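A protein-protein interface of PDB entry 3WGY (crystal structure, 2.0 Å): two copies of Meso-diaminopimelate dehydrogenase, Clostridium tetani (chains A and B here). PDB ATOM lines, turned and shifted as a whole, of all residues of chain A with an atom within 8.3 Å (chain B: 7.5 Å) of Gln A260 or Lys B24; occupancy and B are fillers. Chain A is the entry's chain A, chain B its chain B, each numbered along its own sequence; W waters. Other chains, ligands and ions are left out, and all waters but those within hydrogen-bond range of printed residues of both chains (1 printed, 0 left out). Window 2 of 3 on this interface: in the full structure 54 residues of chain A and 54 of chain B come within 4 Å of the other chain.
Pro A140 touches Gln B25. Gln B25 touches Lys A141 (NE2 to CG, 3.3 Å). NE2 of Gln B25 touches C of Thr A259, at 3.7 Å. Thr A259 touches Ser B282 (CG2 to OG, 3.4 Å). Lys B21 touches Gln A260 (O to CG, 3.2 Å). Lys B24 touches Gln A260. Gln A260 touches Glu B278 (O to OE2, 3.5 Å). Ala A263 touches Ser B275. OE1 of Glu B278 touches CB of Ala A263, 3.8 Å away.
Printed residues of chain B within 4 Å of Pro A140: Gln B25 (3.9 Å). Gln A260 touches just these residues of chain B: Lys B21, Lys B24, Gln B25 and Glu B278. Printed residues of chain B within 4 Å of Gln A265: Ser B275. Of chain A, only Gln A260 (3.4 Å) comes within 4 Å of Lys B24. Met B29 touches none of the printed residues of chain A. Leu B31 touches none of the printed residues of chain A. Printed residues of chain A within 4 Å of Ser B275: Ala A263 and Gln A265. Of the printed residues of chain A, Glu B278 touches Thr A259 (3.0 Å), Gln A260 (3.5 Å) and Ala A263 (3.8 Å). Printed residues of chain A within 4 Å of Ser B282: Thr A259 (3.4 Å). The nearest residue of chain A that does not touch Lys B24 is Lys A141 (5.5 Å).
The backbone carbonyl oxygen (O) of Lys A141 sits at hydrogen-bond distance from the backbone NH (N) of Asn A258, 3.2 Å away. O of Gly A257 lies within hydrogen-bond range of N of Gln A265 (2.9 Å). The backbone carbonyl oxygen (O) of Gly A262 sits close to the side-chain amide oxygen (OD1) of Asn A258 (3.2 Å). The side-chain hydroxyl of Ser B282 sits at hydrogen-bond distance from the backbone carbonyl oxygen of Glu B278.
Water W1 lies within hydrogen-bond range of N of Lys A141, O of Asn A258 and OE1 of Gln B25.
The side-chain amide nitrogen (NE2) of Gln B25 sits at hydrogen-bond distance from the backbone carbonyl oxygen (O) of Asn A258, 3.3 Å away. The side-chain carboxylate of Glu B278 sits at hydrogen-bond distance from the side-chain hydroxyl of Thr A259 (3.0 Å). N of Gln A260 sits close to NE2 of Gln B25, at 3.4 Å. The backbone carbonyl oxygen of Ser B275 is in hydrogen-bond range of the side-chain amide nitrogen of Gln A265 (2.9 Å).
No position is printed for both chains. Of the 13 pairs that touch across the chains among the printed residues, none has its exchanged pair printed and touching as well.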
ATOM      1  N   LEU A 139     -12.500 -19.769 -22.310  1.00  0.00           N
ATOM      2  CA  LEU A 139     -11.879 -19.447 -21.033  1.00  0.00           C
ATOM      3  C   LEU A 139     -12.959 -19.044 -20.025  1.00  0.00           C
ATOM      4  O   LEU A 139     -13.160 -17.861 -19.748  1.00  0.00           O
ATOM      5  CB  LEU A 139     -10.875 -18.306 -21.229  1.00  0.00           C
ATOM      6  CG  LEU A 139      -9.747 -18.638 -22.213  1.00  0.00           C
ATOM      7  CD1 LEU A 139      -8.926 -17.401 -22.529  1.00  0.00           C
ATOM      8  CD2 LEU A 139      -8.867 -19.729 -21.610  1.00  0.00           C
ATOM      9  N   PRO A 140     -13.672 -20.032 -19.466  1.00  0.00           N
ATOM     10  CA  PRO A 140     -14.732 -19.772 -18.490  1.00  0.00           C
ATOM     11  C   PRO A 140     -14.234 -19.008 -17.268  1.00  0.00           C
ATOM     12  O   PRO A 140     -15.005 -18.320 -16.608  1.00  0.00           O
ATOM     13  CB  PRO A 140     -15.247 -21.173 -18.160  1.00  0.00           C
ATOM     14  CG  PRO A 140     -14.055 -22.036 -18.382  1.00  0.00           C
ATOM     15  CD  PRO A 140     -13.489 -21.481 -19.659  1.00  0.00           C
ATOM     16  N   LYS A 141     -12.944 -19.122 -16.975  1.00  0.00           N
ATOM     17  CA  LYS A 141     -12.367 -18.414 -15.840  1.00  0.00           C
ATOM     18  C   LYS A 141     -11.571 -17.223 -16.353  1.00  0.00           C
ATOM     19  O   LYS A 141     -10.378 -17.323 -16.633  1.00  0.00           O
ATOM     20  CB  LYS A 141     -11.464 -19.347 -15.027  1.00  0.00           C
ATOM     21  CG  LYS A 141     -12.165 -20.599 -14.530  1.00  0.00           C
ATOM     22  CD  LYS A 141     -13.360 -20.260 -13.653  1.00  0.00           C
ATOM     23  CE  LYS A 141     -14.190 -21.505 -13.366  1.00  0.00           C
ATOM     24  NZ  LYS A 141     -15.400 -21.200 -12.554  1.00  0.00           N
ATOM     25  N   GLY A 257      -8.013 -14.468 -19.580  1.00  0.00           N
ATOM     26  CA  GLY A 257      -8.275 -15.490 -18.595  1.00  0.00           C
ATOM     27  C   GLY A 257      -7.039 -16.252 -18.182  1.00  0.00           C
ATOM     28  O   GLY A 257      -5.938 -16.041 -18.695  1.00  0.00           O
ATOM     29  N   ASN A 258      -7.231 -17.151 -17.231  1.00  0.00           N
ATOM     30  CA  ASN A 258      -6.150 -17.977 -16.723  1.00  0.00           C
ATOM     31  C   ASN A 258      -6.668 -19.408 -16.704  1.00  0.00           C
ATOM     32  O   ASN A 258      -7.834 -19.653 -16.387  1.00  0.00           O
ATOM     33  CB  ASN A 258      -5.779 -17.548 -15.297  1.00  0.00           C
ATOM     34  CG  ASN A 258      -5.248 -16.126 -15.228  1.00  0.00           C
ATOM     35  OD1 ASN A 258      -4.038 -15.895 -15.292  1.00  0.00           O
ATOM     36  ND2 ASN A 258      -6.157 -15.163 -15.107  1.00  0.00           N
ATOM     37  N   THR A 259      -5.812 -20.350 -17.069  1.00  0.00           N
ATOM     38  CA  THR A 259      -6.196 -21.753 -17.055  1.00  0.00           C
ATOM     39  C   THR A 259      -5.759 -22.277 -15.692  1.00  0.00           C
ATOM     40  O   THR A 259      -4.990 -21.607 -15.003  1.00  0.00           O
ATOM     41  CB  THR A 259      -5.480 -22.529 -18.186  1.00  0.00           C
ATOM     42  OG1 THR A 259      -4.163 -21.991 -18.381  1.00  0.00           O
ATOM     43  CG2 THR A 259      -6.275 -22.434 -19.490  1.00  0.00           C
ATOM     44  N   GLN A 260      -6.254 -23.442 -15.282  1.00  0.00           N
ATOM     45  CA  GLN A 260      -5.857 -24.012 -13.991  1.00  0.00           C
ATOM     46  C   GLN A 260      -4.346 -23.848 -13.830  1.00  0.00           C
ATOM     47  O   GLN A 260      -3.574 -24.379 -14.630  1.00  0.00           O
ATOM     48  CB  GLN A 260      -6.201 -25.507 -13.931  1.00  0.00           C
ATOM     49  CG  GLN A 260      -7.628 -25.850 -13.508  1.00  0.00           C
ATOM     50  CD  GLN A 260      -7.861 -25.683 -12.013  1.00  0.00           C
ATOM     51  OE1 GLN A 260      -8.335 -24.640 -11.554  1.00  0.00           O
ATOM     52  NE2 GLN A 260      -7.513 -26.713 -11.243  1.00  0.00           N
ATOM     53  N   GLY A 261      -3.920 -23.106 -12.814  1.00  0.00           N
ATOM     54  CA  GLY A 261      -2.492 -22.927 -12.616  1.00  0.00           C
ATOM     55  C   GLY A 261      -1.975 -21.506 -12.753  1.00  0.00           C
ATOM     56  O   GLY A 261      -0.831 -21.233 -12.390  1.00  0.00           O
ATOM     57  N   GLY A 262      -2.795 -20.605 -13.290  1.00  0.00           N
ATOM     58  CA  GLY A 262      -2.378 -19.220 -13.426  1.00  0.00           C
ATOM     59  C   GLY A 262      -1.784 -18.778 -14.753  1.00  0.00           C
ATOM     60  O   GLY A 262      -1.394 -17.619 -14.890  1.00  0.00           O
ATOM     61  N   ALA A 263      -1.711 -19.670 -15.734  1.00  0.00           N
ATOM     62  CA  ALA A 263      -1.145 -19.304 -17.033  1.00  0.00           C
ATOM     63  C   ALA A 263      -1.993 -18.236 -17.727  1.00  0.00           C
ATOM     64  O   ALA A 263      -3.201 -18.411 -17.891  1.00  0.00           O
ATOM     65  CB  ALA A 263      -1.030 -20.541 -17.921  1.00  0.00           C
ATOM     66  N   GLN A 265      -3.728 -16.375 -20.509  1.00  0.00           N
ATOM     67  CA  GLN A 265      -4.249 -16.673 -21.844  1.00  0.00           C
ATOM     68  C   GLN A 265      -5.106 -15.500 -22.313  1.00  0.00           C
ATOM     69  O   GLN A 265      -6.086 -15.136 -21.651  1.00  0.00           O
ATOM     70  CB  GLN A 265      -5.107 -17.944 -21.806  1.00  0.00           C
ATOM     71  CG  GLN A 265      -4.504 -19.098 -21.013  1.00  0.00           C
ATOM     72  CD  GLN A 265      -3.365 -19.796 -21.741  1.00  0.00           C
ATOM     73  OE1 GLN A 265      -2.419 -19.159 -22.207  1.00  0.00           O
ATOM     74  NE2 GLN A 265      -3.448 -21.112 -21.832  1.00  0.00           N
ATOM     75  N   LYS B  17      -3.316 -33.970 -19.681  1.00  0.00           N
ATOM     76  CA  LYS B  17      -3.214 -33.326 -18.373  1.00  0.00           C
ATOM     77  C   LYS B  17      -3.921 -31.974 -18.403  1.00  0.00           C
ATOM     78  O   LYS B  17      -4.582 -31.586 -17.440  1.00  0.00           O
ATOM     79  CB  LYS B  17      -1.744 -33.119 -17.980  1.00  0.00           C
ATOM     80  CG  LYS B  17      -1.018 -34.366 -17.528  1.00  0.00           C
ATOM     81  CD  LYS B  17       0.416 -34.030 -17.142  1.00  0.00           C
ATOM     82  CE  LYS B  17       1.096 -35.193 -16.434  1.00  0.00           C
ATOM     83  NZ  LYS B  17       1.088 -36.448 -17.241  1.00  0.00           N
ATOM     84  N   GLY B  18      -3.773 -31.256 -19.513  1.00  0.00           N
ATOM     85  CA  GLY B  18      -4.423 -29.964 -19.649  1.00  0.00           C
ATOM     86  C   GLY B  18      -5.936 -30.104 -19.668  1.00  0.00           C
ATOM     87  O   GLY B  18      -6.656 -29.259 -19.129  1.00  0.00           O
ATOM     88  N   VAL B  19      -6.420 -31.173 -20.294  1.00  0.00           N
ATOM     89  CA  VAL B  19      -7.855 -31.422 -20.374  1.00  0.00           C
ATOM     90  C   VAL B  19      -8.414 -31.720 -18.990  1.00  0.00           C
ATOM     91  O   VAL B  19      -9.470 -31.209 -18.612  1.00  0.00           O
ATOM     92  CB  VAL B  19      -8.164 -32.608 -21.307  1.00  0.00           C
ATOM     93  CG1 VAL B  19      -9.633 -32.985 -21.206  1.00  0.00           C
ATOM     94  CG2 VAL B  19      -7.826 -32.233 -22.736  1.00  0.00           C
ATOM     95  N   GLU B  20      -7.702 -32.556 -18.236  1.00  0.00           N
ATOM     96  CA  GLU B  20      -8.137 -32.906 -16.892  1.00  0.00           C
ATOM     97  C   GLU B  20      -8.284 -31.639 -16.066  1.00  0.00           C
ATOM     98  O   GLU B  20      -9.240 -31.487 -15.310  1.00  0.00           O
ATOM     99  CB  GLU B  20      -7.125 -33.841 -16.224  1.00  0.00           C
ATOM    100  CG  GLU B  20      -7.360 -34.043 -14.731  1.00  0.00           C
ATOM    101  CD  GLU B  20      -6.395 -35.038 -14.123  1.00  0.00           C
ATOM    102  OE1 GLU B  20      -5.172 -34.923 -14.376  1.00  0.00           O
ATOM    103  OE2 GLU B  20      -6.859 -35.929 -13.388  1.00  0.00           O
ATOM    104  N   LYS B  21      -7.329 -30.728 -16.220  1.00  0.00           N
ATOM    105  CA  LYS B  21      -7.353 -29.465 -15.495  1.00  0.00           C
ATOM    106  C   LYS B  21      -8.546 -28.604 -15.883  1.00  0.00           C
ATOM    107  O   LYS B  21      -9.282 -28.125 -15.023  1.00  0.00           O
ATOM    108  CB  LYS B  21      -6.061 -28.683 -15.745  1.00  0.00           C
ATOM    109  CG  LYS B  21      -5.083 -28.786 -14.604  1.00  0.00           C
ATOM    110  CD  LYS B  21      -3.689 -28.319 -14.982  1.00  0.00           C
ATOM    111  CE  LYS B  21      -2.663 -29.142 -14.209  1.00  0.00           C
ATOM    112  NZ  LYS B  21      -1.273 -28.614 -14.283  1.00  0.00           N
ATOM    113  N   ALA B  22      -8.737 -28.414 -17.180  1.00  0.00           N
ATOM    114  CA  ALA B  22      -9.832 -27.593 -17.662  1.00  0.00           C
ATOM    115  C   ALA B  22     -11.199 -28.109 -17.217  1.00  0.00           C
ATOM    116  O   ALA B  22     -12.104 -27.320 -16.939  1.00  0.00           O
ATOM    117  CB  ALA B  22      -9.775 -27.497 -19.177  1.00  0.00           C
ATOM    118  N   ILE B  23     -11.354 -29.426 -17.149  1.00  0.00           N
ATOM    119  CA  ILE B  23     -12.623 -29.994 -16.739  1.00  0.00           C
ATOM    120  C   ILE B  23     -12.986 -29.531 -15.332  1.00  0.00           C
ATOM    121  O   ILE B  23     -14.157 -29.504 -14.973  1.00  0.00           O
ATOM    122  CB  ILE B  23     -12.593 -31.537 -16.806  1.00  0.00           C
ATOM    123  CG1 ILE B  23     -12.538 -31.987 -18.267  1.00  0.00           C
ATOM    124  CG2 ILE B  23     -13.834 -32.116 -16.154  1.00  0.00           C
ATOM    125  CD1 ILE B  23     -12.428 -33.477 -18.443  1.00  0.00           C
ATOM    126  N   LYS B  24     -11.984 -29.148 -14.546  1.00  0.00           N
ATOM    127  CA  LYS B  24     -12.223 -28.667 -13.185  1.00  0.00           C
ATOM    128  C   LYS B  24     -12.847 -27.271 -13.202  1.00  0.00           C
ATOM    129  O   LYS B  24     -13.489 -26.860 -12.229  1.00  0.00           O
ATOM    130  CB  LYS B  24     -10.915 -28.629 -12.387  1.00  0.00           C
ATOM    131  CG  LYS B  24     -10.263 -29.992 -12.164  1.00  0.00           C
ATOM    132  CD  LYS B  24      -8.932 -29.836 -11.437  1.00  0.00           C
ATOM    133  CE  LYS B  24      -8.266 -31.181 -11.191  1.00  0.00           C
ATOM    134  NZ  LYS B  24      -9.071 -32.042 -10.277  1.00  0.00           N
ATOM    135  N   GLN B  25     -12.646 -26.547 -14.305  1.00  0.00           N
ATOM    136  CA  GLN B  25     -13.200 -25.202 -14.466  1.00  0.00           C
ATOM    137  C   GLN B  25     -14.613 -25.261 -15.051  1.00  0.00           C
ATOM    138  O   GLN B  25     -15.215 -24.227 -15.325  1.00  0.00           O
ATOM    139  CB  GLN B  25     -12.320 -24.353 -15.401  1.00  0.00           C
ATOM    140  CG  GLN B  25     -10.876 -24.186 -14.966  1.00  0.00           C
ATOM    141  CD  GLN B  25     -10.125 -23.157 -15.802  1.00  0.00           C
ATOM    142  OE1 GLN B  25     -10.192 -23.165 -17.036  1.00  0.00           O
ATOM    143  NE2 GLN B  25      -9.393 -22.271 -15.131  1.00  0.00           N
ATOM    144  N   ASN B  26     -15.136 -26.470 -15.238  1.00  0.00           N
ATOM    145  CA  ASN B  26     -16.464 -26.645 -15.816  1.00  0.00           C
ATOM    146  C   ASN B  26     -17.411 -27.460 -14.939  1.00  0.00           C
ATOM    147  O   ASN B  26     -17.478 -28.687 -15.036  1.00  0.00           O
ATOM    148  CB  ASN B  26     -16.331 -27.291 -17.192  1.00  0.00           C
ATOM    149  CG  ASN B  26     -15.588 -26.404 -18.179  1.00  0.00           C
ATOM    150  OD1 ASN B  26     -16.197 -25.665 -18.953  1.00  0.00           O
ATOM    151  ND2 ASN B  26     -14.266 -26.461 -18.140  1.00  0.00           N
ATOM    152  N   ASP B  27     -18.157 -26.755 -14.097  1.00  0.00           N
ATOM    153  CA  ASP B  27     -19.105 -27.369 -13.178  1.00  0.00           C
ATOM    154  C   ASP B  27     -20.103 -28.359 -13.778  1.00  0.00           C
ATOM    155  O   ASP B  27     -20.634 -29.203 -13.060  1.00  0.00           O
ATOM    156  CB  ASP B  27     -19.871 -26.277 -12.425  1.00  0.00           C
ATOM    157  CG  ASP B  27     -18.988 -25.508 -11.458  1.00  0.00           C
ATOM    158  OD1 ASP B  27     -18.441 -26.140 -10.527  1.00  0.00           O
ATOM    159  OD2 ASP B  27     -18.836 -24.277 -11.627  1.00  0.00           O
ATOM    160  N   MET B  29     -19.375 -30.617 -16.012  1.00  0.00           N
ATOM    161  CA  MET B  29     -18.654 -31.791 -16.501  1.00  0.00           C
ATOM    162  C   MET B  29     -18.011 -32.603 -15.392  1.00  0.00           C
ATOM    163  O   MET B  29     -17.728 -32.095 -14.303  1.00  0.00           O
ATOM    164  CB  MET B  29     -17.564 -31.380 -17.482  1.00  0.00           C
ATOM    165  CG  MET B  29     -18.078 -30.862 -18.792  1.00  0.00           C
ATOM    166  SD  MET B  29     -16.691 -30.324 -19.802  1.00  0.00           S
ATOM    167  CE  MET B  29     -17.552 -29.389 -21.071  1.00  0.00           C
ATOM    168  N   LEU B  31     -14.982 -35.843 -14.988  1.00  0.00           N
ATOM    169  CA  LEU B  31     -14.006 -36.708 -15.632  1.00  0.00           C
ATOM    170  C   LEU B  31     -14.291 -38.123 -15.152  1.00  0.00           C
ATOM    171  O   LEU B  31     -14.292 -38.383 -13.955  1.00  0.00           O
ATOM    172  CB  LEU B  31     -12.583 -36.304 -15.241  1.00  0.00           C
ATOM    173  CG  LEU B  31     -11.463 -37.143 -15.866  1.00  0.00           C
ATOM    174  CD1 LEU B  31     -11.650 -37.234 -17.380  1.00  0.00           C
ATOM    175  CD2 LEU B  31     -10.115 -36.515 -15.525  1.00  0.00           C
ATOM    176  N   SER B 275       0.535 -20.572 -22.153  1.00  0.00           N
ATOM    177  CA  SER B 275       0.544 -22.025 -22.168  1.00  0.00           C
ATOM    178  C   SER B 275      -0.293 -22.550 -23.333  1.00  0.00           C
ATOM    179  O   SER B 275      -1.511 -22.722 -23.217  1.00  0.00           O
ATOM    180  CB  SER B 275      -0.004 -22.561 -20.847  1.00  0.00           C
ATOM    181  OG  SER B 275       0.017 -23.974 -20.826  1.00  0.00           O
ATOM    182  N   GLU B 278      -2.403 -25.871 -22.616  1.00  0.00           N
ATOM    183  CA  GLU B 278      -3.577 -25.710 -21.773  1.00  0.00           C
ATOM    184  C   GLU B 278      -4.697 -24.959 -22.493  1.00  0.00           C
ATOM    185  O   GLU B 278      -5.878 -25.114 -22.164  1.00  0.00           O
ATOM    186  CB  GLU B 278      -3.207 -24.985 -20.484  1.00  0.00           C
ATOM    187  CG  GLU B 278      -2.161 -25.722 -19.669  1.00  0.00           C
ATOM    188  CD  GLU B 278      -2.217 -25.349 -18.208  1.00  0.00           C
ATOM    189  OE1 GLU B 278      -2.089 -24.148 -17.882  1.00  0.00           O
ATOM    190  OE2 GLU B 278      -2.402 -26.266 -17.384  1.00  0.00           O
ATOM    191  N   SER B 282      -8.434 -26.306 -23.226  1.00  0.00           N
ATOM    192  CA  SER B 282      -9.659 -25.588 -22.882  1.00  0.00           C
ATOM    193  C   SER B 282     -10.600 -25.603 -24.072  1.00  0.00           C
ATOM    194  O   SER B 282     -11.814 -25.747 -23.917  1.00  0.00           O
ATOM    195  CB  SER B 282      -9.361 -24.134 -22.506  1.00  0.00           C
ATOM    196  OG  SER B 282      -8.689 -24.068 -21.272  1.00  0.00           O
ATOM    197  N   VAL B 285     -12.163 -29.023 -24.349  1.00  0.00           N
ATOM    198  CA  VAL B 285     -13.226 -29.187 -23.369  1.00  0.00           C
ATOM    199  C   VAL B 285     -14.507 -28.458 -23.767  1.00  0.00           C
ATOM    200  O   VAL B 285     -15.590 -29.040 -23.702  1.00  0.00           O
ATOM    201  CB  VAL B 285     -12.787 -28.699 -21.983  1.00  0.00           C
ATOM    202  CG1 VAL B 285     -13.968 -28.757 -21.009  1.00  0.00           C
ATOM    203  CG2 VAL B 285     -11.641 -29.570 -21.478  1.00  0.00           C
HETATM  204  O   HOH W   1     -10.557 -20.042 -17.972  1.00  0.00           O
